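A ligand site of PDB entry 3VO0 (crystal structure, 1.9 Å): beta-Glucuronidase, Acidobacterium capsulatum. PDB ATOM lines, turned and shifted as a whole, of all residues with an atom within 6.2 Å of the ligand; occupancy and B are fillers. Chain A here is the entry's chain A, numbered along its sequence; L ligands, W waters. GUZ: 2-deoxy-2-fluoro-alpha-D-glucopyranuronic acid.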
ATOM      1  N   GLU A  45      26.135  -1.982  18.169  1.00  0.00           N
ATOM      2  CA  GLU A  45      27.205  -2.218  17.195  1.00  0.00           C
ATOM      3  C   GLU A  45      27.615  -0.951  16.473  1.00  0.00           C
ATOM      4  O   GLU A  45      26.745  -0.193  15.970  1.00  0.00           O
ATOM      5  CB  GLU A  45      26.709  -3.207  16.137  1.00  0.00           C
ATOM      6  CG  GLU A  45      26.458  -4.629  16.635  1.00  0.00           C
ATOM      7  CD  GLU A  45      27.680  -5.293  17.191  1.00  0.00           C
ATOM      8  OE1 GLU A  45      28.818  -4.895  16.802  1.00  0.00           O
ATOM      9  OE2 GLU A  45      27.508  -6.220  18.039  1.00  0.00           O
ATOM     10  N   ARG A  76      26.657   3.540  24.466  1.00  0.00           N
ATOM     11  CA  ARG A  76      27.960   2.999  24.049  1.00  0.00           C
ATOM     12  C   ARG A  76      27.823   2.388  22.648  1.00  0.00           C
ATOM     13  O   ARG A  76      26.880   1.614  22.356  1.00  0.00           O
ATOM     14  CB  ARG A  76      28.479   1.956  25.070  1.00  0.00           C
ATOM     15  CG  ARG A  76      29.861   1.296  24.748  1.00  0.00           C
ATOM     16  CD  ARG A  76      29.664  -0.058  24.092  1.00  0.00           C
ATOM     17  NE  ARG A  76      30.918  -0.708  23.706  1.00  0.00           N
ATOM     18  CZ  ARG A  76      31.061  -1.976  23.365  1.00  0.00           C
ATOM     19  NH1 ARG A  76      30.026  -2.818  23.368  1.00  0.00           N
ATOM     20  NH2 ARG A  76      32.269  -2.429  23.012  1.00  0.00           N
ATOM     21  N   GLY A  78      30.228   0.254  19.978  1.00  0.00           N
ATOM     22  CA  GLY A  78      31.439  -0.564  19.719  1.00  0.00           C
ATOM     23  C   GLY A  78      31.106  -1.959  19.260  1.00  0.00           C
ATOM     24  O   GLY A  78      30.509  -2.161  18.178  1.00  0.00           O
ATOM     25  N   GLY A  79      31.490  -2.965  20.041  1.00  0.00           N
ATOM     26  CA  GLY A  79      31.156  -4.336  19.698  1.00  0.00           C
ATOM     27  C   GLY A  79      32.054  -4.969  18.651  1.00  0.00           C
ATOM     28  O   GLY A  79      33.010  -4.338  18.196  1.00  0.00           O
ATOM     29  N   ASN A  80      31.730  -6.210  18.268  1.00  0.00           N
ATOM     30  CA  ASN A  80      32.527  -6.950  17.290  1.00  0.00           C
ATOM     31  C   ASN A  80      32.635  -6.208  15.948  1.00  0.00           C
ATOM     32  O   ASN A  80      33.642  -6.366  15.249  1.00  0.00           O
ATOM     33  CB  ASN A  80      31.941  -8.334  17.032  1.00  0.00           C
ATOM     34  CG  ASN A  80      32.085  -9.270  18.236  1.00  0.00           C
ATOM     35  OD1 ASN A  80      32.834  -8.990  19.151  1.00  0.00           O
ATOM     36  ND2 ASN A  80      31.345 -10.358  18.222  1.00  0.00           N
ATOM     37  N   THR A  81      31.619  -5.413  15.597  1.00  0.00           N
ATOM     38  CA  THR A  81      31.662  -4.693  14.318  1.00  0.00           C
ATOM     39  C   THR A  81      32.607  -3.486  14.340  1.00  0.00           C
ATOM     40  O   THR A  81      32.962  -2.968  13.264  1.00  0.00           O
ATOM     41  CB  THR A  81      30.246  -4.250  13.808  1.00  0.00           C
ATOM     42  OG1 THR A  81      29.686  -3.349  14.732  1.00  0.00           O
ATOM     43  CG2 THR A  81      29.320  -5.446  13.619  1.00  0.00           C
ATOM     44  N   GLY A 103      21.686  -5.548  14.168  1.00  0.00           N
ATOM     45  CA  GLY A 103      21.447  -6.298  15.408  1.00  0.00           C
ATOM     46  C   GLY A 103      22.782  -6.711  16.049  1.00  0.00           C
ATOM     47  O   GLY A 103      23.840  -6.607  15.399  1.00  0.00           O
ATOM     48  N   PRO A 104      22.748  -7.165  17.311  1.00  0.00           N
ATOM     49  CA  PRO A 104      23.998  -7.596  17.962  1.00  0.00           C
ATOM     50  C   PRO A 104      24.744  -8.542  17.051  1.00  0.00           C
ATOM     51  O   PRO A 104      24.117  -9.402  16.432  1.00  0.00           O
ATOM     52  CB  PRO A 104      23.483  -8.310  19.218  1.00  0.00           C
ATOM     53  CG  PRO A 104      22.273  -7.487  19.584  1.00  0.00           C
ATOM     54  CD  PRO A 104      21.605  -7.249  18.242  1.00  0.00           C
ATOM     55  N   ASP A 105      26.064  -8.368  16.944  1.00  0.00           N
ATOM     56  CA  ASP A 105      26.893  -9.299  16.140  1.00  0.00           C
ATOM     57  C   ASP A 105      26.792 -10.732  16.696  1.00  0.00           C
ATOM     58  O   ASP A 105      26.897 -10.921  17.913  1.00  0.00           O
ATOM     59  CB  ASP A 105      28.349  -8.841  16.137  1.00  0.00           C
ATOM     60  CG  ASP A 105      29.216  -9.681  15.210  1.00  0.00           C
ATOM     61  OD1 ASP A 105      29.156  -9.459  13.966  1.00  0.00           O
ATOM     62  OD2 ASP A 105      29.931 -10.594  15.742  1.00  0.00           O
ATOM     63  N   LYS A 106      26.609 -11.716  15.814  1.00  0.00           N
ATOM     64  CA  LYS A 106      26.407 -13.090  16.282  1.00  0.00           C
ATOM     65  C   LYS A 106      27.696 -13.841  16.625  1.00  0.00           C
ATOM     66  O   LYS A 106      27.647 -14.951  17.171  1.00  0.00           O
ATOM     67  CB  LYS A 106      25.554 -13.898  15.302  1.00  0.00           C
ATOM     68  CG  LYS A 106      24.176 -13.323  15.105  1.00  0.00           C
ATOM     69  CD  LYS A 106      23.425 -14.106  14.065  1.00  0.00           C
ATOM     70  CE  LYS A 106      21.931 -14.155  14.373  1.00  0.00           C
ATOM     71  NZ  LYS A 106      21.233 -12.969  13.843  1.00  0.00           N
ATOM     72  N   GLY A 107      28.835 -13.232  16.316  1.00  0.00           N
ATOM     73  CA  GLY A 107      30.145 -13.752  16.742  1.00  0.00           C
ATOM     74  C   GLY A 107      30.512 -15.122  16.195  1.00  0.00           C
ATOM     75  O   GLY A 107      31.121 -15.931  16.904  1.00  0.00           O
ATOM     76  N   ASN A 172      37.397  -3.378  20.686  1.00  0.00           N
ATOM     77  CA  ASN A 172      36.416  -4.100  21.470  1.00  0.00           C
ATOM     78  C   ASN A 172      36.923  -5.501  21.829  1.00  0.00           C
ATOM     79  O   ASN A 172      37.370  -6.241  20.945  1.00  0.00           O
ATOM     80  CB  ASN A 172      35.155  -4.238  20.636  1.00  0.00           C
ATOM     81  CG  ASN A 172      34.162  -5.129  21.249  1.00  0.00           C
ATOM     82  OD1 ASN A 172      33.532  -4.766  22.238  1.00  0.00           O
ATOM     83  ND2 ASN A 172      33.991  -6.318  20.683  1.00  0.00           N
ATOM     84  N   GLU A 173      36.797  -5.881  23.111  1.00  0.00           N
ATOM     85  CA  GLU A 173      37.170  -7.229  23.590  1.00  0.00           C
ATOM     86  C   GLU A 173      38.565  -7.640  23.042  1.00  0.00           C
ATOM     87  O   GLU A 173      38.707  -8.660  22.369  1.00  0.00           O
ATOM     88  CB  GLU A 173      36.087  -8.269  23.262  1.00  0.00           C
ATOM     89  CG  GLU A 173      34.665  -7.882  23.768  1.00  0.00           C
ATOM     90  CD  GLU A 173      33.610  -8.978  23.737  1.00  0.00           C
ATOM     91  OE1 GLU A 173      33.666  -9.907  22.900  1.00  0.00           O
ATOM     92  OE2 GLU A 173      32.656  -8.892  24.561  1.00  0.00           O
ATOM     93  N   HIS A 241      33.222  -6.524  30.107  1.00  0.00           N
ATOM     94  CA  HIS A 241      31.952  -7.035  29.669  1.00  0.00           C
ATOM     95  C   HIS A 241      31.466  -8.196  30.519  1.00  0.00           C
ATOM     96  O   HIS A 241      32.224  -8.728  31.349  1.00  0.00           O
ATOM     97  CB  HIS A 241      32.015  -7.432  28.187  1.00  0.00           C
ATOM     98  CG  HIS A 241      32.425  -6.315  27.285  1.00  0.00           C
ATOM     99  ND1 HIS A 241      32.736  -6.507  25.957  1.00  0.00           N
ATOM    100  CD2 HIS A 241      32.588  -4.992  27.516  1.00  0.00           C
ATOM    101  CE1 HIS A 241      33.058  -5.353  25.404  1.00  0.00           C
ATOM    102  NE2 HIS A 241      32.988  -4.419  26.323  1.00  0.00           N
ATOM    103  N   TYR A 243      28.467 -11.615  30.023  1.00  0.00           N
ATOM    104  CA  TYR A 243      27.326 -12.368  29.520  1.00  0.00           C
ATOM    105  C   TYR A 243      27.047 -13.543  30.460  1.00  0.00           C
ATOM    106  O   TYR A 243      27.955 -14.305  30.776  1.00  0.00           O
ATOM    107  CB  TYR A 243      27.568 -12.866  28.064  1.00  0.00           C
ATOM    108  CG  TYR A 243      27.293 -11.751  27.086  1.00  0.00           C
ATOM    109  CD1 TYR A 243      28.229 -10.729  26.892  1.00  0.00           C
ATOM    110  CD2 TYR A 243      26.047 -11.649  26.453  1.00  0.00           C
ATOM    111  CE1 TYR A 243      27.940  -9.634  26.062  1.00  0.00           C
ATOM    112  CE2 TYR A 243      25.756 -10.565  25.591  1.00  0.00           C
ATOM    113  CZ  TYR A 243      26.705  -9.576  25.399  1.00  0.00           C
ATOM    114  OH  TYR A 243      26.417  -8.508  24.593  1.00  0.00           O
ATOM    115  N   GLU A 287      29.472  -3.625  28.117  1.00  0.00           N
ATOM    116  CA  GLU A 287      28.714  -4.515  27.263  1.00  0.00           C
ATOM    117  C   GLU A 287      28.227  -5.710  28.047  1.00  0.00           C
ATOM    118  O   GLU A 287      29.031  -6.474  28.598  1.00  0.00           O
ATOM    119  CB  GLU A 287      29.494  -4.957  26.020  1.00  0.00           C
ATOM    120  CG  GLU A 287      28.656  -5.649  24.956  1.00  0.00           C
ATOM    121  CD  GLU A 287      29.514  -6.496  24.010  1.00  0.00           C
ATOM    122  OE1 GLU A 287      30.676  -6.113  23.797  1.00  0.00           O
ATOM    123  OE2 GLU A 287      28.990  -7.491  23.496  1.00  0.00           O
ATOM    124  N   CYS A 291      22.767 -13.722  27.080  1.00  0.00           N
ATOM    125  CA  CYS A 291      23.412 -14.856  26.413  1.00  0.00           C
ATOM    126  C   CYS A 291      24.205 -14.340  25.224  1.00  0.00           C
ATOM    127  O   CYS A 291      23.682 -13.543  24.423  1.00  0.00           O
ATOM    128  CB  CYS A 291      22.366 -15.869  25.980  1.00  0.00           C
ATOM    129  SG  CYS A 291      22.977 -17.266  24.941  1.00  0.00           S
ATOM    130  N   TYR A 292      25.467 -14.779  25.110  1.00  0.00           N
ATOM    131  CA  TYR A 292      26.308 -14.245  24.033  1.00  0.00           C
ATOM    132  C   TYR A 292      25.976 -14.787  22.640  1.00  0.00           C
ATOM    133  O   TYR A 292      24.979 -15.512  22.454  1.00  0.00           O
ATOM    134  CB  TYR A 292      27.807 -14.331  24.382  1.00  0.00           C
ATOM    135  CG  TYR A 292      28.381 -15.728  24.609  1.00  0.00           C
ATOM    136  CD1 TYR A 292      28.487 -16.642  23.537  1.00  0.00           C
ATOM    137  CD2 TYR A 292      28.891 -16.103  25.866  1.00  0.00           C
ATOM    138  CE1 TYR A 292      29.057 -17.940  23.740  1.00  0.00           C
ATOM    139  CE2 TYR A 292      29.471 -17.391  26.072  1.00  0.00           C
ATOM    140  CZ  TYR A 292      29.553 -18.281  24.997  1.00  0.00           C
ATOM    141  OH  TYR A 292      30.103 -19.543  25.171  1.00  0.00           O
ATOM    142  N   GLN A 293      26.802 -14.428  21.648  1.00  0.00           N
ATOM    143  CA  GLN A 293      26.511 -14.694  20.235  1.00  0.00           C
ATOM    144  C   GLN A 293      25.068 -14.323  19.840  1.00  0.00           C
ATOM    145  O   GLN A 293      24.389 -15.044  19.102  1.00  0.00           O
ATOM    146  CB  GLN A 293      26.869 -16.124  19.859  1.00  0.00           C
ATOM    147  CG  GLN A 293      28.358 -16.319  19.853  1.00  0.00           C
ATOM    148  CD  GLN A 293      28.753 -17.772  19.727  1.00  0.00           C
ATOM    149  OE1 GLN A 293      28.031 -18.689  20.120  1.00  0.00           O
ATOM    150  NE2 GLN A 293      29.906 -17.985  19.131  1.00  0.00           N
ATOM    151  N   GLY A 294      24.627 -13.193  20.353  1.00  0.00           N
ATOM    152  CA  GLY A 294      23.351 -12.625  19.872  1.00  0.00           C
ATOM    153  C   GLY A 294      22.131 -13.078  20.639  1.00  0.00           C
ATOM    154  O   GLY A 294      21.006 -12.722  20.269  1.00  0.00           O
ATOM    155  N   GLY A 295      22.332 -13.848  21.699  1.00  0.00           N
ATOM    156  CA  GLY A 295      21.194 -14.267  22.541  1.00  0.00           C
ATOM    157  C   GLY A 295      20.476 -15.538  22.138  1.00  0.00           C
ATOM    158  O   GLY A 295      20.694 -16.123  21.035  1.00  0.00           O
ATOM    159  N   HIS A 327      23.643  -4.544  25.754  1.00  0.00           N
ATOM    160  CA  HIS A 327      23.820  -4.601  24.314  1.00  0.00           C
ATOM    161  C   HIS A 327      22.502  -4.903  23.606  1.00  0.00           C
ATOM    162  O   HIS A 327      21.609  -5.570  24.165  1.00  0.00           O
ATOM    163  CB  HIS A 327      24.855  -5.686  23.957  1.00  0.00           C
ATOM    164  CG  HIS A 327      25.478  -5.505  22.595  1.00  0.00           C
ATOM    165  ND1 HIS A 327      26.198  -4.387  22.249  1.00  0.00           N
ATOM    166  CD2 HIS A 327      25.564  -6.352  21.533  1.00  0.00           C
ATOM    167  CE1 HIS A 327      26.653  -4.523  21.015  1.00  0.00           C
ATOM    168  NE2 HIS A 327      26.294  -5.705  20.569  1.00  0.00           N
ATOM    169  N   TYR A 334      18.125 -10.605  22.547  1.00  0.00           N
ATOM    170  CA  TYR A 334      18.269  -9.939  23.853  1.00  0.00           C
ATOM    171  C   TYR A 334      18.096  -8.421  23.838  1.00  0.00           C
ATOM    172  O   TYR A 334      18.283  -7.768  24.838  1.00  0.00           O
ATOM    173  CB  TYR A 334      19.546 -10.350  24.561  1.00  0.00           C
ATOM    174  CG  TYR A 334      20.879 -10.026  23.877  1.00  0.00           C
ATOM    175  CD1 TYR A 334      21.198  -8.736  23.447  1.00  0.00           C
ATOM    176  CD2 TYR A 334      21.861 -11.027  23.731  1.00  0.00           C
ATOM    177  CE1 TYR A 334      22.442  -8.444  22.840  1.00  0.00           C
ATOM    178  CE2 TYR A 334      23.095 -10.744  23.164  1.00  0.00           C
ATOM    179  CZ  TYR A 334      23.389  -9.467  22.724  1.00  0.00           C
ATOM    180  OH  TYR A 334      24.609  -9.210  22.157  1.00  0.00           O
HETATM  181  C1  GUZ L   1      29.809  -8.320  22.639  1.00  0.00           C
HETATM  182  C2  GUZ L   1      30.278  -8.026  21.218  1.00  0.00           C
HETATM  183  F2  GUZ L   1      31.014  -6.864  21.274  1.00  0.00           F
HETATM  184  C3  GUZ L   1      29.056  -7.835  20.356  1.00  0.00           C
HETATM  185  O3  GUZ L   1      29.458  -7.545  19.024  1.00  0.00           O
HETATM  186  C4  GUZ L   1      28.236  -9.124  20.426  1.00  0.00           C
HETATM  187  O4  GUZ L   1      26.981  -8.971  19.790  1.00  0.00           O
HETATM  188  C5  GUZ L   1      28.008  -9.589  21.869  1.00  0.00           C
HETATM  189  C6  GUZ L   1      27.413 -10.998  21.889  1.00  0.00           C
HETATM  190  O6A GUZ L   1      28.213 -11.968  21.869  1.00  0.00           O
HETATM  191  O6B GUZ L   1      26.166 -11.144  21.911  1.00  0.00           O
HETATM  192  O5  GUZ L   1      29.221  -9.586  22.619  1.00  0.00           O
HETATM  193  O   HOH W   1      30.726 -12.063  20.665  1.00  0.00           O
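Water W1 lies within hydrogen-bond range of O6A of the ligand (2.8 Å) and ND2 of Asn 80 (3.0 Å).
The side-chain carboxylate (OE2) of Glu 287 sits at hydrogen-bond distance from the side-chain hydroxyl (OH) of Tyr 243 (3.0 Å).
The backbone NH (N) of Asp 105 lies within hydrogen-bond range of the side-chain carboxylate (OE2) of Glu 45 (2.8 Å).
The side-chain carboxylate (OE2) of Glu 45 is in hydrogen-bond range of a ring nitrogen (NE2) of His 327, 2.9 Å away.
OE1 of Glu 45 lies within hydrogen-bond range of OG1 of Thr 81, 2.7 Å away.
OD2 of Asp 105 lies within hydrogen-bond range of ND2 of Asn 80.
OD2 of Asp 105 lies within hydrogen-bond range of N of Gly 107, at 2.9 Å.
NE2 of Gln 293 is in hydrogen-bond range of O of Gly 107 (3.3 Å).
The guanidinium group (NH2) of Arg 76 sits at hydrogen-bond distance from the side-chain amide oxygen (OD1) of Asn 172.
The side-chain carboxylate of Glu 287 is bonded to a carbon (C1) of the ligand, 1.4 Å away.
O6B of the ligand sits at hydrogen-bond distance from OH of Tyr 334 (2.5 Å).
OE2 of Glu 45 lies within hydrogen-bond range of O3 of the ligand (2.6 Å).
N of Asp 105 sits at hydrogen-bond distance from O4 of the ligand.
O of Asp 105 is in hydrogen-bond range of O4 of the ligand, at 2.7 Å.
N of Asn 80 lies within hydrogen-bond range of O3 of the ligand.
An oxygen (O3) of the ligand lies close to the side-chain amide nitrogen (ND2) of Asn 80 (3.5 Å).
N of Gln 293 is in hydrogen-bond range of O6A of the ligand, at 2.8 Å.
The backbone NH (N) of Gly 294 is in hydrogen-bond range of an oxygen (O6B) of the ligand, 3.0 Å away.
A ring nitrogen (NE2) of His 327 is in hydrogen-bond range of an oxygen (O4) of the ligand.
A fluorine (F2) of the ligand lies close to the side-chain amide nitrogen of Asn 172 (3.1 Å).
CA of Gly 79 touches F2 of the ligand, at 3.0 Å.
Pro 104 touches the ligand (C to O4, 3.6 Å).
Glu 173 touches the ligand.
Tyr 243 touches the ligand.
Tyr 292 touches the ligand (CB to O6A, 3.5 Å).
Hydrophobic or aromatic side chains within 4 Å of the ligand: Pro 104, Tyr 243, Tyr 292, His 327 and Tyr 334.
Within 4 Å of the ligand: Glu 45, Gly 79, Asn 80, Pro 104, Asp 105, Asn 172, Glu 173, Tyr 243, Glu 287, Tyr 292, Gln 293, Gly 294, His 327 and Tyr 334.
The nearest printed residue that does not touch the ligand is Cys 291 (4.3 Å).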
